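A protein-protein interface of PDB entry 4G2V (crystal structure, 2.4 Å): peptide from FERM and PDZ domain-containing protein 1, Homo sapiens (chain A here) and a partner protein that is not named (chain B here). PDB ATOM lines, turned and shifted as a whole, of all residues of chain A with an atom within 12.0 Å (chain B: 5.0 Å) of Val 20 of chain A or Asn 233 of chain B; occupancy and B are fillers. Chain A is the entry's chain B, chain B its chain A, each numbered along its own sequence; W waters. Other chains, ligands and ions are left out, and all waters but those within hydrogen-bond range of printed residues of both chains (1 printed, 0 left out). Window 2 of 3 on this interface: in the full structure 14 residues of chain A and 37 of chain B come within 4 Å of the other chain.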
ATOM      1  N   VAL A  20     -24.663  10.772  31.969  1.00  0.00           N
ATOM      2  CA  VAL A  20     -24.947   9.744  32.967  1.00  0.00           C
ATOM      3  C   VAL A  20     -26.106   8.840  32.553  1.00  0.00           C
ATOM      4  O   VAL A  20     -27.261   9.272  32.520  1.00  0.00           O
ATOM      5  CB  VAL A  20     -25.230  10.384  34.321  1.00  0.00           C
ATOM      6  N   MET A  21     -25.791   7.587  32.235  1.00  0.00           N
ATOM      7  CA  MET A  21     -26.812   6.592  31.932  1.00  0.00           C
ATOM      8  C   MET A  21     -27.472   6.104  33.209  1.00  0.00           C
ATOM      9  O   MET A  21     -26.795   5.634  34.124  1.00  0.00           O
ATOM     10  CB  MET A  21     -26.214   5.384  31.216  1.00  0.00           C
ATOM     11  CG  MET A  21     -25.535   5.676  29.900  1.00  0.00           C
ATOM     12  SD  MET A  21     -25.440   4.169  28.915  1.00  0.00           S
ATOM     13  CE  MET A  21     -25.159   2.947  30.194  1.00  0.00           C
ATOM     14  N   GLU A  22     -28.795   6.196  33.266  1.00  0.00           N
ATOM     15  CA  GLU A  22     -29.522   5.687  34.415  1.00  0.00           C
ATOM     16  C   GLU A  22     -29.992   4.264  34.129  1.00  0.00           C
ATOM     17  O   GLU A  22     -30.899   4.041  33.327  1.00  0.00           O
ATOM     18  CB  GLU A  22     -30.709   6.598  34.721  1.00  0.00           C
ATOM     19  CG  GLU A  22     -30.316   8.048  34.978  1.00  0.00           C
ATOM     20  CD  GLU A  22     -29.719   8.249  36.356  1.00  0.00           C
ATOM     21  OE1 GLU A  22     -29.780   7.303  37.172  1.00  0.00           O
ATOM     22  OE2 GLU A  22     -29.191   9.350  36.625  1.00  0.00           O
ATOM     23  N   MET A  23     -29.356   3.303  34.793  1.00  0.00           N
ATOM     24  CA  MET A  23     -29.680   1.892  34.636  1.00  0.00           C
ATOM     25  C   MET A  23     -30.862   1.451  35.493  1.00  0.00           C
ATOM     26  O   MET A  23     -31.166   2.057  36.522  1.00  0.00           O
ATOM     27  CB  MET A  23     -28.462   1.021  34.951  1.00  0.00           C
ATOM     28  CG  MET A  23     -27.229   1.364  34.129  1.00  0.00           C
ATOM     29  SD  MET A  23     -27.458   1.091  32.360  1.00  0.00           S
ATOM     30  CE  MET A  23     -27.627  -0.690  32.314  1.00  0.00           C
ATOM     31  N   GLU A  24     -31.524   0.389  35.049  1.00  0.00           N
ATOM     32  CA  GLU A  24     -32.456  -0.347  35.888  1.00  0.00           C
ATOM     33  C   GLU A  24     -31.683  -1.334  36.768  1.00  0.00           C
ATOM     34  O   GLU A  24     -30.628  -1.839  36.373  1.00  0.00           O
ATOM     35  CB  GLU A  24     -33.482  -1.076  35.020  1.00  0.00           C
ATOM     36  CG  GLU A  24     -34.298  -0.128  34.157  1.00  0.00           C
ATOM     37  CD  GLU A  24     -35.019   0.919  34.990  1.00  0.00           C
ATOM     38  OE1 GLU A  24     -35.722   0.527  35.944  1.00  0.00           O
ATOM     39  OE2 GLU A  24     -34.869   2.127  34.708  1.00  0.00           O
ATOM     40  N   TYR B 196     -28.148   3.064  23.088  1.00  0.00           N
ATOM     41  CA  TYR B 196     -27.472   4.337  23.270  1.00  0.00           C
ATOM     42  C   TYR B 196     -25.951   4.180  23.120  1.00  0.00           C
ATOM     43  O   TYR B 196     -25.318   4.914  22.357  1.00  0.00           O
ATOM     44  CB  TYR B 196     -27.853   4.915  24.635  1.00  0.00           C
ATOM     45  CG  TYR B 196     -27.176   6.214  25.000  1.00  0.00           C
ATOM     46  CD1 TYR B 196     -27.719   7.435  24.617  1.00  0.00           C
ATOM     47  CD2 TYR B 196     -26.004   6.221  25.748  1.00  0.00           C
ATOM     48  CE1 TYR B 196     -27.106   8.626  24.959  1.00  0.00           C
ATOM     49  CE2 TYR B 196     -25.384   7.402  26.095  1.00  0.00           C
ATOM     50  CZ  TYR B 196     -25.940   8.603  25.699  1.00  0.00           C
ATOM     51  OH  TYR B 196     -25.324   9.781  26.043  1.00  0.00           O
ATOM     52  N   SER B 229     -34.174  11.465  31.895  1.00  0.00           N
ATOM     53  CA  SER B 229     -32.738  11.708  31.775  1.00  0.00           C
ATOM     54  C   SER B 229     -32.186  11.016  30.541  1.00  0.00           C
ATOM     55  O   SER B 229     -31.495  11.632  29.725  1.00  0.00           O
ATOM     56  CB  SER B 229     -31.985  11.212  33.012  1.00  0.00           C
ATOM     57  OG  SER B 229     -32.227  12.038  34.134  1.00  0.00           O
ATOM     58  N   ASN B 230     -32.498   9.729  30.420  1.00  0.00           N
ATOM     59  CA  ASN B 230     -32.017   8.910  29.313  1.00  0.00           C
ATOM     60  C   ASN B 230     -32.489   9.413  27.947  1.00  0.00           C
ATOM     61  O   ASN B 230     -31.731   9.386  26.979  1.00  0.00           O
ATOM     62  CB  ASN B 230     -32.390   7.435  29.536  1.00  0.00           C
ATOM     63  CG  ASN B 230     -31.614   6.808  30.693  1.00  0.00           C
ATOM     64  OD1 ASN B 230     -30.446   7.134  30.919  1.00  0.00           O
ATOM     65  ND2 ASN B 230     -32.264   5.918  31.437  1.00  0.00           N
ATOM     66  N   LEU B 231     -33.733   9.888  27.876  1.00  0.00           N
ATOM     67  CA  LEU B 231     -34.258  10.469  26.640  1.00  0.00           C
ATOM     68  C   LEU B 231     -33.531  11.763  26.285  1.00  0.00           C
ATOM     69  O   LEU B 231     -33.185  11.999  25.125  1.00  0.00           O
ATOM     70  CB  LEU B 231     -35.764  10.715  26.754  1.00  0.00           C
ATOM     71  CG  LEU B 231     -36.631   9.453  26.720  1.00  0.00           C
ATOM     72  CD1 LEU B 231     -37.951   9.684  27.437  1.00  0.00           C
ATOM     73  CD2 LEU B 231     -36.852   8.977  25.289  1.00  0.00           C
ATOM     74  N   GLY B 232     -33.300  12.598  27.292  1.00  0.00           N
ATOM     75  CA  GLY B 232     -32.531  13.812  27.101  1.00  0.00           C
ATOM     76  C   GLY B 232     -31.183  13.518  26.471  1.00  0.00           C
ATOM     77  O   GLY B 232     -30.768  14.196  25.531  1.00  0.00           O
ATOM     78  N   ASN B 233     -30.507  12.492  26.984  1.00  0.00           N
ATOM     79  CA  ASN B 233     -29.187  12.113  26.487  1.00  0.00           C
ATOM     80  C   ASN B 233     -29.198  11.716  25.015  1.00  0.00           C
ATOM     81  O   ASN B 233     -28.341  12.143  24.242  1.00  0.00           O
ATOM     82  CB  ASN B 233     -28.592  10.978  27.326  1.00  0.00           C
ATOM     83  CG  ASN B 233     -28.353  11.379  28.770  1.00  0.00           C
ATOM     84  OD1 ASN B 233     -28.234  12.563  29.089  1.00  0.00           O
ATOM     85  ND2 ASN B 233     -28.272  10.388  29.652  1.00  0.00           N
ATOM     86  N   ALA B 234     -30.166  10.888  24.633  1.00  0.00           N
ATOM     87  CA  ALA B 234     -30.280  10.437  23.249  1.00  0.00           C
ATOM     88  C   ALA B 234     -30.535  11.596  22.279  1.00  0.00           C
ATOM     89  O   ALA B 234     -29.983  11.624  21.179  1.00  0.00           O
ATOM     90  CB  ALA B 234     -31.367   9.384  23.124  1.00  0.00           C
ATOM     91  N   TYR B 235     -31.373  12.545  22.682  1.00  0.00           N
ATOM     92  CA  TYR B 235     -31.679  13.689  21.825  1.00  0.00           C
ATOM     93  C   TYR B 235     -30.486  14.630  21.657  1.00  0.00           C
ATOM     94  O   TYR B 235     -30.399  15.359  20.668  1.00  0.00           O
ATOM     95  CB  TYR B 235     -32.904  14.448  22.337  1.00  0.00           C
ATOM     96  CG  TYR B 235     -34.213  13.751  22.038  1.00  0.00           C
ATOM     97  CD1 TYR B 235     -34.724  13.716  20.745  1.00  0.00           C
ATOM     98  CD2 TYR B 235     -34.941  13.136  23.046  1.00  0.00           C
ATOM     99  CE1 TYR B 235     -35.924  13.081  20.467  1.00  0.00           C
ATOM    100  CE2 TYR B 235     -36.140  12.498  22.779  1.00  0.00           C
ATOM    101  CZ  TYR B 235     -36.628  12.475  21.489  1.00  0.00           C
ATOM    102  OH  TYR B 235     -37.825  11.842  21.224  1.00  0.00           O
ATOM    103  N   ILE B 236     -29.571  14.617  22.618  1.00  0.00           N
ATOM    104  CA  ILE B 236     -28.322  15.353  22.471  1.00  0.00           C
ATOM    105  C   ILE B 236     -27.551  14.825  21.268  1.00  0.00           C
ATOM    106  O   ILE B 236     -27.145  15.590  20.391  1.00  0.00           O
ATOM    107  CB  ILE B 236     -27.437  15.238  23.726  1.00  0.00           C
ATOM    108  CG1 ILE B 236     -28.035  16.056  24.872  1.00  0.00           C
ATOM    109  CG2 ILE B 236     -26.015  15.705  23.423  1.00  0.00           C
ATOM    110  CD1 ILE B 236     -28.171  17.541  24.559  1.00  0.00           C
ATOM    111  N   PHE B 237     -27.368  13.508  21.225  1.00  0.00           N
ATOM    112  CA  PHE B 237     -26.646  12.868  20.131  1.00  0.00           C
ATOM    113  C   PHE B 237     -27.459  12.805  18.840  1.00  0.00           C
ATOM    114  O   PHE B 237     -26.908  12.558  17.768  1.00  0.00           O
ATOM    115  CB  PHE B 237     -26.172  11.473  20.539  1.00  0.00           C
ATOM    116  CG  PHE B 237     -25.020  11.489  21.497  1.00  0.00           C
ATOM    117  CD1 PHE B 237     -23.717  11.457  21.030  1.00  0.00           C
ATOM    118  CD2 PHE B 237     -25.237  11.554  22.864  1.00  0.00           C
ATOM    119  CE1 PHE B 237     -22.646  11.479  21.913  1.00  0.00           C
ATOM    120  CE2 PHE B 237     -24.175  11.579  23.751  1.00  0.00           C
ATOM    121  CZ  PHE B 237     -22.876  11.541  23.273  1.00  0.00           C
ATOM    122  N   TYR B 248     -34.930  17.482  30.184  1.00  0.00           N
ATOM    123  CA  TYR B 248     -34.160  17.833  31.369  1.00  0.00           C
ATOM    124  C   TYR B 248     -34.993  18.723  32.288  1.00  0.00           C
ATOM    125  O   TYR B 248     -34.949  18.580  33.511  1.00  0.00           O
ATOM    126  CB  TYR B 248     -32.838  18.503  30.983  1.00  0.00           C
ATOM    127  CG  TYR B 248     -31.835  17.551  30.354  1.00  0.00           C
ATOM    128  CD1 TYR B 248     -31.717  16.240  30.800  1.00  0.00           C
ATOM    129  CD2 TYR B 248     -31.012  17.962  29.310  1.00  0.00           C
ATOM    130  CE1 TYR B 248     -30.801  15.365  30.229  1.00  0.00           C
ATOM    131  CE2 TYR B 248     -30.096  17.097  28.732  1.00  0.00           C
ATOM    132  CZ  TYR B 248     -29.995  15.798  29.196  1.00  0.00           C
ATOM    133  OH  TYR B 248     -29.088  14.932  28.624  1.00  0.00           O
ATOM    134  N   GLN B 266     -27.716  17.782  39.232  1.00  0.00           N
ATOM    135  CA  GLN B 266     -27.452  17.079  37.983  1.00  0.00           C
ATOM    136  C   GLN B 266     -28.317  17.641  36.850  1.00  0.00           C
ATOM    137  O   GLN B 266     -27.810  17.975  35.778  1.00  0.00           O
ATOM    138  CB  GLN B 266     -27.702  15.579  38.177  1.00  0.00           C
ATOM    139  CG  GLN B 266     -27.628  14.734  36.912  1.00  0.00           C
ATOM    140  CD  GLN B 266     -28.066  13.294  37.150  1.00  0.00           C
ATOM    141  OE1 GLN B 266     -28.001  12.791  38.273  1.00  0.00           O
ATOM    142  NE2 GLN B 266     -28.522  12.629  36.091  1.00  0.00           N
HETATM  143  O   HOH W   1     -33.333   3.087  32.709  1.00  0.00           O
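The backbone carbonyl oxygen (O) of Glu 22 of chain A is in hydrogen-bond range of the side-chain amide nitrogen (ND2) of Asn 230 of chain B (3.0 Å).
ND2 of Asn 233 of chain B is in hydrogen-bond range of O of Val 20 of chain A, 3.2 Å away.
OE2 of Glu 22 of chain A is in hydrogen-bond range of NE2 of Gln 266 of chain B, 3.4 Å away.
O of Ser 229 of chain B sits close to OD1 of Asn 233 of chain B (3.5 Å).
The side-chain amide oxygen (OD1) of Asn 233 of chain B lies within hydrogen-bond range of the side-chain hydroxyl (OH) of Tyr 248 of chain B (2.6 Å).
CD2 of Tyr 196 of chain B touches SD of Met 21 of chain A, at 3.8 Å.
Met 21 of chain A touches Asn 230 of chain B (CA to OD1, 3.8 Å).
Of chain B, only Asn 233 (3.2 Å) comes within 4 Å of Val 20 of chain A.
Asn 233 of chain B touches one residue of chain A.
No residue of chain A comes within 4 Å of Ser 229 of chain B.
Asn 230 of chain B touches just these residues of chain A: Met 21 and Glu 22.
No residue of chain A comes within 4 Å of Gly 232 of chain B.
Ala 234 of chain B touches none of the printed residues of chain A.
No residue of chain A comes within 4 Å of Phe 237 of chain B.
Printed residues of chain A within 4 Å of Gln 266 of chain B: Glu 22 (3.4 Å).
Printed residues of chain A within 4 Å of Tyr 196 of chain B: Met 21.
Printed residues of chain B within 4 Å of Glu 22 of chain A: Asn 230 and Gln 266.
Of the printed residues of chain B, Met 21 of chain A touches Tyr 196 and Asn 230.
Leu 231 of chain B touches none of the printed residues of chain A.
Glu 24 of chain A touches none of the printed residues of chain B.
The nearest printed residue of chain A that does not touch Gln 266 of chain B is Val 20 of chain A (4.4 Å).
Of the 12 printed residues of chain B, 4 touch a printed residue of chain A.
Hydrophobic or aromatic side chains of chain B within 4 Å of the printed part of chain A: Tyr 196.
Of the 5 printed residues of chain A, 3 touch a printed residue of chain B.
Printed residues of chain A that touch a printed residue of chain B: Val 20, Met 21 and Glu 22.
Hydrophobic or aromatic side chains of chain A within 4 Å of the printed part of chain B: Met 21.
Water W1 lies within hydrogen-bond range of the backbone carbonyl oxygen (O) of Glu 22 of chain A (2.7 Å), the side-chain carboxylate (OE2) of Glu 24 of chain A (2.7 Å) and the side-chain amide nitrogen (ND2) of Asn 230 of chain B (3.3 Å).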
